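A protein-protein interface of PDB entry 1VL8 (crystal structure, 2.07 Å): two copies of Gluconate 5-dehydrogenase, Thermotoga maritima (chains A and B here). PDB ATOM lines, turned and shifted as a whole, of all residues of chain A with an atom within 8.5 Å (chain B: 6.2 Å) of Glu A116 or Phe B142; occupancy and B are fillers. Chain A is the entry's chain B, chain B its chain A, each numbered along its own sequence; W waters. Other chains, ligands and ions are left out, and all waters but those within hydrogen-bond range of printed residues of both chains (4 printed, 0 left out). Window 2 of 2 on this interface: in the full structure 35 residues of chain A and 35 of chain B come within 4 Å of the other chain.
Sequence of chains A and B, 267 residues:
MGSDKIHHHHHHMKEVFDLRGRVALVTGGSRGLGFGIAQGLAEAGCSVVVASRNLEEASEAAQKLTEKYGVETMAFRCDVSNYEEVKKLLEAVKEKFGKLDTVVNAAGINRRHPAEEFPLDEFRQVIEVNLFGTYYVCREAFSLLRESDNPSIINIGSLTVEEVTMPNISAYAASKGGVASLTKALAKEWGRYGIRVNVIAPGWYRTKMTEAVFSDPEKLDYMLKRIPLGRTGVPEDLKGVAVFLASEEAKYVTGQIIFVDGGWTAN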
ATOM      1  N   HIS A 113     -38.470  12.040  19.178  1.00  0.00           N
ATOM      2  CA  HIS A 113     -37.579  12.907  18.426  1.00  0.00           C
ATOM      3  C   HIS A 113     -36.183  12.310  18.470  1.00  0.00           C
ATOM      4  O   HIS A 113     -35.829  11.676  19.453  1.00  0.00           O
ATOM      5  CB  HIS A 113     -37.474  14.308  19.064  1.00  0.00           C
ATOM      6  CG  HIS A 113     -38.779  14.985  19.289  1.00  0.00           C
ATOM      7  ND1 HIS A 113     -39.430  15.687  18.298  1.00  0.00           N
ATOM      8  CD2 HIS A 113     -39.574  15.045  20.389  1.00  0.00           C
ATOM      9  CE1 HIS A 113     -40.572  16.155  18.783  1.00  0.00           C
ATOM     10  NE2 HIS A 113     -40.683  15.770  20.049  1.00  0.00           N
ATOM     11  N   PRO A 114     -35.364  12.584  17.448  1.00  0.00           N
ATOM     12  CA  PRO A 114     -33.953  12.268  17.567  1.00  0.00           C
ATOM     13  C   PRO A 114     -33.356  12.967  18.804  1.00  0.00           C
ATOM     14  O   PRO A 114     -33.686  14.136  19.065  1.00  0.00           O
ATOM     15  CB  PRO A 114     -33.344  12.835  16.284  1.00  0.00           C
ATOM     16  CG  PRO A 114     -34.480  12.934  15.300  1.00  0.00           C
ATOM     17  CD  PRO A 114     -35.678  13.257  16.172  1.00  0.00           C
ATOM     18  N   ALA A 115     -32.529  12.250  19.568  1.00  0.00           N
ATOM     19  CA  ALA A 115     -31.988  12.770  20.848  1.00  0.00           C
ATOM     20  C   ALA A 115     -31.234  14.101  20.660  1.00  0.00           C
ATOM     21  O   ALA A 115     -31.305  14.983  21.504  1.00  0.00           O
ATOM     22  CB  ALA A 115     -31.089  11.747  21.515  1.00  0.00           C
ATOM     23  N   GLU A 116     -30.560  14.247  19.520  1.00  0.00           N
ATOM     24  CA  GLU A 116     -29.777  15.441  19.248  1.00  0.00           C
ATOM     25  C   GLU A 116     -30.643  16.655  18.898  1.00  0.00           C
ATOM     26  O   GLU A 116     -30.147  17.739  18.911  1.00  0.00           O
ATOM     27  CB  GLU A 116     -28.705  15.168  18.201  1.00  0.00           C
ATOM     28  CG  GLU A 116     -29.168  14.937  16.750  1.00  0.00           C
ATOM     29  CD  GLU A 116     -29.576  13.482  16.422  1.00  0.00           C
ATOM     30  OE1 GLU A 116     -29.804  12.625  17.294  1.00  0.00           O
ATOM     31  OE2 GLU A 116     -29.701  13.186  15.238  1.00  0.00           O
ATOM     32  N   GLU A 117     -31.924  16.452  18.603  1.00  0.00           N
ATOM     33  CA  GLU A 117     -32.870  17.504  18.273  1.00  0.00           C
ATOM     34  C   GLU A 117     -34.034  17.566  19.279  1.00  0.00           C
ATOM     35  O   GLU A 117     -34.926  18.367  19.098  1.00  0.00           O
ATOM     36  CB  GLU A 117     -33.487  17.234  16.887  1.00  0.00           C
ATOM     37  CG  GLU A 117     -32.471  17.029  15.750  1.00  0.00           C
ATOM     38  CD  GLU A 117     -33.052  16.248  14.515  1.00  0.00           C
ATOM     39  OE1 GLU A 117     -34.308  16.079  14.411  1.00  0.00           O
ATOM     40  OE2 GLU A 117     -32.238  15.813  13.651  1.00  0.00           O
ATOM     41  N   PHE A 118     -34.055  16.707  20.294  1.00  0.00           N
ATOM     42  CA  PHE A 118     -35.183  16.614  21.244  1.00  0.00           C
ATOM     43  C   PHE A 118     -35.444  17.980  21.905  1.00  0.00           C
ATOM     44  O   PHE A 118     -34.524  18.569  22.481  1.00  0.00           O
ATOM     45  CB  PHE A 118     -34.875  15.561  22.309  1.00  0.00           C
ATOM     46  CG  PHE A 118     -36.061  14.782  22.783  1.00  0.00           C
ATOM     47  CD1 PHE A 118     -37.057  15.393  23.529  1.00  0.00           C
ATOM     48  CD2 PHE A 118     -36.178  13.453  22.494  1.00  0.00           C
ATOM     49  CE1 PHE A 118     -38.164  14.676  23.957  1.00  0.00           C
ATOM     50  CE2 PHE A 118     -37.272  12.713  22.934  1.00  0.00           C
ATOM     51  CZ  PHE A 118     -38.254  13.313  23.668  1.00  0.00           C
ATOM     52  N   PRO A 119     -36.671  18.541  21.745  1.00  0.00           N
ATOM     53  CA  PRO A 119     -36.945  19.838  22.407  1.00  0.00           C
ATOM     54  C   PRO A 119     -36.841  19.655  23.908  1.00  0.00           C
ATOM     55  O   PRO A 119     -37.336  18.668  24.459  1.00  0.00           O
ATOM     56  CB  PRO A 119     -38.364  20.202  21.969  1.00  0.00           C
ATOM     57  CG  PRO A 119     -38.614  19.378  20.737  1.00  0.00           C
ATOM     58  CD  PRO A 119     -37.800  18.103  20.903  1.00  0.00           C
ATOM     59  N   LEU A 120     -36.160  20.584  24.552  1.00  0.00           N
ATOM     60  CA  LEU A 120     -35.778  20.402  25.951  1.00  0.00           C
ATOM     61  C   LEU A 120     -36.988  20.398  26.867  1.00  0.00           C
ATOM     62  O   LEU A 120     -37.043  19.617  27.806  1.00  0.00           O
ATOM     63  CB  LEU A 120     -34.711  21.428  26.345  1.00  0.00           C
ATOM     64  CG  LEU A 120     -33.507  21.071  25.473  1.00  0.00           C
ATOM     65  CD1 LEU A 120     -32.837  22.248  25.018  1.00  0.00           C
ATOM     66  CD2 LEU A 120     -32.598  19.995  26.152  1.00  0.00           C
ATOM     67  N   PHE A 123     -38.438  16.970  26.553  1.00  0.00           N
ATOM     68  CA  PHE A 123     -37.598  15.980  27.226  1.00  0.00           C
ATOM     69  C   PHE A 123     -37.897  15.930  28.735  1.00  0.00           C
ATOM     70  O   PHE A 123     -38.153  14.862  29.307  1.00  0.00           O
ATOM     71  CB  PHE A 123     -36.114  16.312  26.998  1.00  0.00           C
ATOM     72  CG  PHE A 123     -35.219  15.264  27.482  1.00  0.00           C
ATOM     73  CD1 PHE A 123     -34.867  15.195  28.840  1.00  0.00           C
ATOM     74  CD2 PHE A 123     -34.749  14.269  26.607  1.00  0.00           C
ATOM     75  CE1 PHE A 123     -34.023  14.163  29.294  1.00  0.00           C
ATOM     76  CE2 PHE A 123     -33.925  13.249  27.064  1.00  0.00           C
ATOM     77  CZ  PHE A 123     -33.564  13.189  28.412  1.00  0.00           C
ATOM     78  N   ASN A 168     -35.468   7.389  18.856  1.00  0.00           N
ATOM     79  CA  ASN A 168     -36.256   8.592  19.136  1.00  0.00           C
ATOM     80  C   ASN A 168     -37.040   8.630  20.412  1.00  0.00           C
ATOM     81  O   ASN A 168     -37.943   9.458  20.530  1.00  0.00           O
ATOM     82  CB  ASN A 168     -37.157   8.943  17.930  1.00  0.00           C
ATOM     83  CG  ASN A 168     -36.356   9.145  16.684  1.00  0.00           C
ATOM     84  OD1 ASN A 168     -35.165   9.469  16.746  1.00  0.00           O
ATOM     85  ND2 ASN A 168     -36.965   8.899  15.542  1.00  0.00           N
ATOM     86  N   SER A 170     -35.451   8.705  23.744  1.00  0.00           N
ATOM     87  CA  SER A 170     -34.439   8.933  24.799  1.00  0.00           C
ATOM     88  C   SER A 170     -35.059   9.358  26.142  1.00  0.00           C
ATOM     89  O   SER A 170     -34.723   8.784  27.179  1.00  0.00           O
ATOM     90  CB  SER A 170     -33.346   9.962  24.367  1.00  0.00           C
ATOM     91  OG  SER A 170     -33.845  11.245  23.981  1.00  0.00           O
ATOM     92  N   LEU B  90     -19.972  23.773  25.651  1.00  0.00           N
ATOM     93  CA  LEU B  90     -19.584  23.118  24.393  1.00  0.00           C
ATOM     94  C   LEU B  90     -19.085  24.066  23.335  1.00  0.00           C
ATOM     95  O   LEU B  90     -18.186  23.689  22.574  1.00  0.00           O
ATOM     96  CB  LEU B  90     -20.698  22.183  23.859  1.00  0.00           C
ATOM     97  CG  LEU B  90     -20.660  20.740  24.417  1.00  0.00           C
ATOM     98  CD1 LEU B  90     -19.396  19.922  24.092  1.00  0.00           C
ATOM     99  CD2 LEU B  90     -20.953  20.692  25.968  1.00  0.00           C
ATOM    100  N   TYR B 135     -27.880  14.339  30.069  1.00  0.00           N
ATOM    101  CA  TYR B 135     -28.492  14.496  28.751  1.00  0.00           C
ATOM    102  C   TYR B 135     -28.052  15.779  27.982  1.00  0.00           C
ATOM    103  O   TYR B 135     -27.656  15.706  26.784  1.00  0.00           O
ATOM    104  CB  TYR B 135     -30.035  14.376  28.798  1.00  0.00           C
ATOM    105  CG  TYR B 135     -30.635  14.770  27.473  1.00  0.00           C
ATOM    106  CD1 TYR B 135     -30.385  14.013  26.321  1.00  0.00           C
ATOM    107  CD2 TYR B 135     -31.377  15.946  27.345  1.00  0.00           C
ATOM    108  CE1 TYR B 135     -30.858  14.407  25.070  1.00  0.00           C
ATOM    109  CE2 TYR B 135     -31.901  16.321  26.124  1.00  0.00           C
ATOM    110  CZ  TYR B 135     -31.631  15.551  24.988  1.00  0.00           C
ATOM    111  OH  TYR B 135     -32.092  15.977  23.793  1.00  0.00           O
ATOM    112  N   VAL B 137     -25.443  17.632  28.209  1.00  0.00           N
ATOM    113  CA  VAL B 137     -24.032  17.572  27.785  1.00  0.00           C
ATOM    114  C   VAL B 137     -23.912  16.677  26.533  1.00  0.00           C
ATOM    115  O   VAL B 137     -23.305  17.075  25.542  1.00  0.00           O
ATOM    116  CB  VAL B 137     -23.095  17.080  28.898  1.00  0.00           C
ATOM    117  CG1 VAL B 137     -21.647  16.881  28.378  1.00  0.00           C
ATOM    118  CG2 VAL B 137     -23.068  18.069  30.121  1.00  0.00           C
ATOM    119  N   CYS B 138     -24.490  15.475  26.601  1.00  0.00           N
ATOM    120  CA  CYS B 138     -24.509  14.567  25.447  1.00  0.00           C
ATOM    121  C   CYS B 138     -25.089  15.240  24.200  1.00  0.00           C
ATOM    122  O   CYS B 138     -24.490  15.160  23.102  1.00  0.00           O
ATOM    123  CB  CYS B 138     -25.324  13.313  25.778  1.00  0.00           C
ATOM    124  SG  CYS B 138     -24.553  12.247  27.001  1.00  0.00           S
ATOM    125  N   ARG B 139     -26.259  15.881  24.380  1.00  0.00           N
ATOM    126  CA  ARG B 139     -26.977  16.570  23.298  1.00  0.00           C
ATOM    127  C   ARG B 139     -26.079  17.653  22.626  1.00  0.00           C
ATOM    128  O   ARG B 139     -25.943  17.715  21.402  1.00  0.00           O
ATOM    129  CB  ARG B 139     -28.274  17.189  23.864  1.00  0.00           C
ATOM    130  CG  ARG B 139     -29.244  17.730  22.843  1.00  0.00           C
ATOM    131  CD  ARG B 139     -30.277  18.596  23.561  1.00  0.00           C
ATOM    132  NE  ARG B 139     -31.441  18.928  22.732  1.00  0.00           N
ATOM    133  CZ  ARG B 139     -31.450  19.942  21.857  1.00  0.00           C
ATOM    134  NH1 ARG B 139     -30.371  20.704  21.697  1.00  0.00           N
ATOM    135  NH2 ARG B 139     -32.542  20.217  21.164  1.00  0.00           N
ATOM    136  N   GLU B 140     -25.444  18.484  23.444  1.00  0.00           N
ATOM    137  CA  GLU B 140     -24.654  19.574  22.933  1.00  0.00           C
ATOM    138  C   GLU B 140     -23.312  19.158  22.397  1.00  0.00           C
ATOM    139  O   GLU B 140     -22.758  19.870  21.572  1.00  0.00           O
ATOM    140  CB  GLU B 140     -24.516  20.683  23.984  1.00  0.00           C
ATOM    141  CG  GLU B 140     -25.867  21.230  24.459  1.00  0.00           C
ATOM    142  CD  GLU B 140     -26.718  21.728  23.309  1.00  0.00           C
ATOM    143  OE1 GLU B 140     -26.384  22.777  22.711  1.00  0.00           O
ATOM    144  OE2 GLU B 140     -27.700  21.043  22.979  1.00  0.00           O
ATOM    145  N   ALA B 141     -22.789  18.018  22.856  1.00  0.00           N
ATOM    146  CA  ALA B 141     -21.529  17.458  22.399  1.00  0.00           C
ATOM    147  C   ALA B 141     -21.660  16.740  21.064  1.00  0.00           C
ATOM    148  O   ALA B 141     -20.682  16.531  20.376  1.00  0.00           O
ATOM    149  CB  ALA B 141     -20.987  16.453  23.443  1.00  0.00           C
ATOM    150  N   PHE B 142     -22.879  16.359  20.709  1.00  0.00           N
ATOM    151  CA  PHE B 142     -23.151  15.581  19.506  1.00  0.00           C
ATOM    152  C   PHE B 142     -22.452  16.135  18.246  1.00  0.00           C
ATOM    153  O   PHE B 142     -21.798  15.402  17.528  1.00  0.00           O
ATOM    154  CB  PHE B 142     -24.671  15.469  19.269  1.00  0.00           C
ATOM    155  CG  PHE B 142     -25.031  14.701  18.045  1.00  0.00           C
ATOM    156  CD1 PHE B 142     -25.018  13.318  18.052  1.00  0.00           C
ATOM    157  CD2 PHE B 142     -25.380  15.355  16.879  1.00  0.00           C
ATOM    158  CE1 PHE B 142     -25.353  12.598  16.900  1.00  0.00           C
ATOM    159  CE2 PHE B 142     -25.707  14.666  15.742  1.00  0.00           C
ATOM    160  CZ  PHE B 142     -25.700  13.281  15.748  1.00  0.00           C
ATOM    161  N   SER B 143     -22.634  17.415  17.961  1.00  0.00           N
ATOM    162  CA  SER B 143     -22.139  17.951  16.714  1.00  0.00           C
ATOM    163  C   SER B 143     -20.617  17.841  16.556  1.00  0.00           C
ATOM    164  O   SER B 143     -20.136  17.584  15.440  1.00  0.00           O
ATOM    165  CB  SER B 143     -22.555  19.395  16.603  1.00  0.00           C
ATOM    166  OG  SER B 143     -21.989  20.154  17.646  1.00  0.00           O
ATOM    167  N   LEU B 144     -19.870  18.017  17.653  1.00  0.00           N
ATOM    168  CA  LEU B 144     -18.412  17.741  17.630  1.00  0.00           C
ATOM    169  C   LEU B 144     -18.052  16.264  17.614  1.00  0.00           C
ATOM    170  O   LEU B 144     -17.120  15.870  16.942  1.00  0.00           O
ATOM    171  CB  LEU B 144     -17.681  18.409  18.810  1.00  0.00           C
ATOM    172  CG  LEU B 144     -17.515  19.921  18.748  1.00  0.00           C
ATOM    173  CD1 LEU B 144     -16.986  20.479  20.061  1.00  0.00           C
ATOM    174  CD2 LEU B 144     -16.612  20.304  17.601  1.00  0.00           C
ATOM    175  N   LEU B 145     -18.751  15.464  18.421  1.00  0.00           N
ATOM    176  CA  LEU B 145     -18.508  14.034  18.478  1.00  0.00           C
ATOM    177  C   LEU B 145     -18.679  13.361  17.115  1.00  0.00           C
ATOM    178  O   LEU B 145     -17.917  12.454  16.766  1.00  0.00           O
ATOM    179  CB  LEU B 145     -19.406  13.344  19.534  1.00  0.00           C
ATOM    180  CG  LEU B 145     -19.038  13.617  20.992  1.00  0.00           C
ATOM    181  CD1 LEU B 145     -20.066  13.062  21.895  1.00  0.00           C
ATOM    182  CD2 LEU B 145     -17.679  13.046  21.323  1.00  0.00           C
ATOM    183  N   ARG B 146     -19.677  13.823  16.354  1.00  0.00           N
ATOM    184  CA  ARG B 146     -19.906  13.412  14.954  1.00  0.00           C
ATOM    185  C   ARG B 146     -18.724  13.612  14.044  1.00  0.00           C
ATOM    186  O   ARG B 146     -18.631  12.982  13.009  1.00  0.00           O
ATOM    187  CB  ARG B 146     -20.963  14.290  14.300  1.00  0.00           C
ATOM    188  CG  ARG B 146     -22.330  13.983  14.604  1.00  0.00           C
ATOM    189  CD  ARG B 146     -22.785  12.702  13.943  1.00  0.00           C
ATOM    190  NE  ARG B 146     -22.778  12.625  12.473  1.00  0.00           N
ATOM    191  CZ  ARG B 146     -23.612  13.252  11.636  1.00  0.00           C
ATOM    192  NH1 ARG B 146     -24.510  14.163  12.041  1.00  0.00           N
ATOM    193  NH2 ARG B 146     -23.508  12.982  10.344  1.00  0.00           N
ATOM    194  N   GLU B 147     -17.889  14.583  14.359  1.00  0.00           N
ATOM    195  CA  GLU B 147     -16.708  14.853  13.546  1.00  0.00           C
ATOM    196  C   GLU B 147     -15.496  14.041  13.972  1.00  0.00           C
ATOM    197  O   GLU B 147     -14.495  14.074  13.296  1.00  0.00           O
ATOM    198  CB  GLU B 147     -16.382  16.345  13.593  1.00  0.00           C
ATOM    199  CG  GLU B 147     -17.552  17.186  13.233  1.00  0.00           C
ATOM    200  CD  GLU B 147     -17.281  18.686  13.313  1.00  0.00           C
ATOM    201  OE1 GLU B 147     -16.264  19.136  13.901  1.00  0.00           O
ATOM    202  OE2 GLU B 147     -18.131  19.418  12.758  1.00  0.00           O
ATOM    203  N   LEU B 186     -29.076   6.391  23.702  1.00  0.00           N
ATOM    204  CA  LEU B 186     -28.076   7.086  22.897  1.00  0.00           C
ATOM    205  C   LEU B 186     -27.206   6.149  22.104  1.00  0.00           C
ATOM    206  O   LEU B 186     -26.835   6.461  20.942  1.00  0.00           O
ATOM    207  CB  LEU B 186     -27.225   7.995  23.773  1.00  0.00           C
ATOM    208  CG  LEU B 186     -27.995   9.121  24.488  1.00  0.00           C
ATOM    209  CD1 LEU B 186     -27.059   9.998  25.370  1.00  0.00           C
ATOM    210  CD2 LEU B 186     -28.816  10.006  23.531  1.00  0.00           C
ATOM    211  N   GLU B 189     -29.243   5.075  19.132  1.00  0.00           N
ATOM    212  CA  GLU B 189     -29.478   6.107  18.086  1.00  0.00           C
ATOM    213  C   GLU B 189     -28.189   6.568  17.390  1.00  0.00           C
ATOM    214  O   GLU B 189     -28.179   6.876  16.204  1.00  0.00           O
ATOM    215  CB  GLU B 189     -30.140   7.350  18.701  1.00  0.00           C
ATOM    216  CG  GLU B 189     -31.597   7.191  19.037  1.00  0.00           C
ATOM    217  CD  GLU B 189     -32.209   8.439  19.634  1.00  0.00           C
ATOM    218  OE1 GLU B 189     -31.912   9.556  19.133  1.00  0.00           O
ATOM    219  OE2 GLU B 189     -32.994   8.328  20.612  1.00  0.00           O
ATOM    220  N   TRP B 190     -27.118   6.641  18.161  1.00  0.00           N
ATOM    221  CA  TRP B 190     -25.893   7.236  17.679  1.00  0.00           C
ATOM    222  C   TRP B 190     -24.829   6.251  17.223  1.00  0.00           C
ATOM    223  O   TRP B 190     -23.799   6.704  16.722  1.00  0.00           O
ATOM    224  CB  TRP B 190     -25.328   8.237  18.686  1.00  0.00           C
ATOM    225  CG  TRP B 190     -26.202   9.441  18.932  1.00  0.00           C
ATOM    226  CD1 TRP B 190     -27.326   9.820  18.214  1.00  0.00           C
ATOM    227  CD2 TRP B 190     -26.053  10.427  19.972  1.00  0.00           C
ATOM    228  NE1 TRP B 190     -27.865  10.978  18.758  1.00  0.00           N
ATOM    229  CE2 TRP B 190     -27.109  11.376  19.819  1.00  0.00           C
ATOM    230  CE3 TRP B 190     -25.145  10.605  21.021  1.00  0.00           C
ATOM    231  CZ2 TRP B 190     -27.259  12.489  20.667  1.00  0.00           C
ATOM    232  CZ3 TRP B 190     -25.286  11.711  21.832  1.00  0.00           C
ATOM    233  CH2 TRP B 190     -26.338  12.648  21.646  1.00  0.00           C
ATOM    234  N   TYR B 193     -23.483   6.715  13.814  1.00  0.00           N
ATOM    235  CA  TYR B 193     -22.446   7.746  13.629  1.00  0.00           C
ATOM    236  C   TYR B 193     -21.100   7.294  14.228  1.00  0.00           C
ATOM    237  O   TYR B 193     -20.134   8.077  14.339  1.00  0.00           O
ATOM    238  CB  TYR B 193     -22.904   9.065  14.284  1.00  0.00           C
ATOM    239  CG  TYR B 193     -24.220   9.559  13.735  1.00  0.00           C
ATOM    240  CD1 TYR B 193     -24.354   9.835  12.385  1.00  0.00           C
ATOM    241  CD2 TYR B 193     -25.345   9.692  14.545  1.00  0.00           C
ATOM    242  CE1 TYR B 193     -25.572  10.271  11.852  1.00  0.00           C
ATOM    243  CE2 TYR B 193     -26.552  10.116  14.027  1.00  0.00           C
ATOM    244  CZ  TYR B 193     -26.664  10.411  12.678  1.00  0.00           C
ATOM    245  OH  TYR B 193     -27.853  10.842  12.124  1.00  0.00           O
ATOM    246  N   ILE B 195     -20.655   6.704  17.350  1.00  0.00           N
ATOM    247  CA  ILE B 195     -20.532   7.235  18.712  1.00  0.00           C
ATOM    248  C   ILE B 195     -20.912   6.153  19.726  1.00  0.00           C
ATOM    249  O   ILE B 195     -22.040   5.679  19.749  1.00  0.00           O
ATOM    250  CB  ILE B 195     -21.412   8.504  18.929  1.00  0.00           C
ATOM    251  CG1 ILE B 195     -21.115   9.559  17.845  1.00  0.00           C
ATOM    252  CG2 ILE B 195     -21.188   9.076  20.321  1.00  0.00           C
ATOM    253  CD1 ILE B 195     -21.983  10.775  17.966  1.00  0.00           C
HETATM  254  O   HOH W   1     -29.946  10.812  13.759  1.00  0.00           O
HETATM  255  O   HOH W   2     -34.461  10.426  21.525  1.00  0.00           O
HETATM  256  O   HOH W   3     -30.978  10.097  16.654  1.00  0.00           O
HETATM  257  O   HOH W   4     -34.319   6.143  21.585  1.00  0.00           O
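No position is printed for both chains.
Water W1 lies within hydrogen-bond range of the side-chain hydroxyl (OH) of Tyr B193 and the side-chain carboxylate (OE2) of Glu A116. Water W2 lies within hydrogen-bond range of OG of Ser A170 (2.7 Å), OE2 of Glu B189 (2.7 Å), O of His A113 (2.8 Å) and N of Ala A115 (3.3 Å). Water W3 bridges OE1 of Glu B189 and OE1 of Glu A116. Water W4 lies within hydrogen-bond range of the side-chain carboxylate of Glu B189 and the backbone NH of Asn A168.
Among the printed residues, merely in contact across the chains: Phe A118 with Tyr B135, Phe A123 with Tyr B135, Ala A115 with Leu B186, Glu A117 with Arg B139, Glu A116 with Phe B142, Ala A115 with Arg B139, Pro A114 with Glu B189, Leu A120 with Tyr B135, Leu A120 with Arg B139, Glu A116 with Arg B139, Ala A115 with Trp B190 and Ser A170 with Glu B189.
NE of Arg B139 sits close to OH of Tyr B135 (3.2 Å). The guanidinium group (NH1) of Arg B139 lies within salt-bridge range of the side-chain carboxylate (OE2) of Glu B140 (3.0 Å). O of Trp B190 is in hydrogen-bond range of N of Ile B195 (3.2 Å). N of His A113 lies within hydrogen-bond range of O of Asn A168, 3.0 Å away.
The side-chain hydroxyl (OH) of Tyr B135 sits at hydrogen-bond distance from the backbone carbonyl oxygen (O) of Ala A115. NH2 of Arg B139 lies within hydrogen-bond range of O of Phe A118 (2.9 Å). The backbone NH (N) of Ala A115 lies within hydrogen-bond range of the side-chain carboxylate (OE1) of Glu B189 (2.8 Å). OE2 of Glu B189 lies within hydrogen-bond range of N of Asn A168 (3.2 Å). The side-chain carboxylate (OE1) of Glu A116 sits at hydrogen-bond distance from the indole nitrogen (NE1) of Trp B190 (2.9 Å).
Of the 11 printed residues of chain A, 9 touch a printed residue of chain B. Of the 18 printed residues of chain B, 6 touch a printed residue of chain A. Among the printed residues, 17 pairs touch across the chains.
Printed residues of chain B within 4 Å of Ala A115: Tyr B135, Arg B139, Leu B186, Glu B189 and Trp B190. Glu A116 touches just these residues of chain B: Arg B139, Phe B142 and Trp B190. No residue of chain A comes within 4 Å of Ala B141. Leu B144 touches none of the printed residues of chain A. Of the printed residues of chain A, Glu B189 touches Pro A114, Ala A115, Asn A168 and Ser A170. Tyr B193 touches none of the printed residues of chain A. The nearest residue of chain B that does not touch Glu A116 is Glu B189 (4.2 Å). The nearest residue of chain A that does not touch Phe B142 is Ala A115 (6.8 Å). The nearest printed residue of chain B that does not touch Pro A114 is Tyr B135 (5.3 Å).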
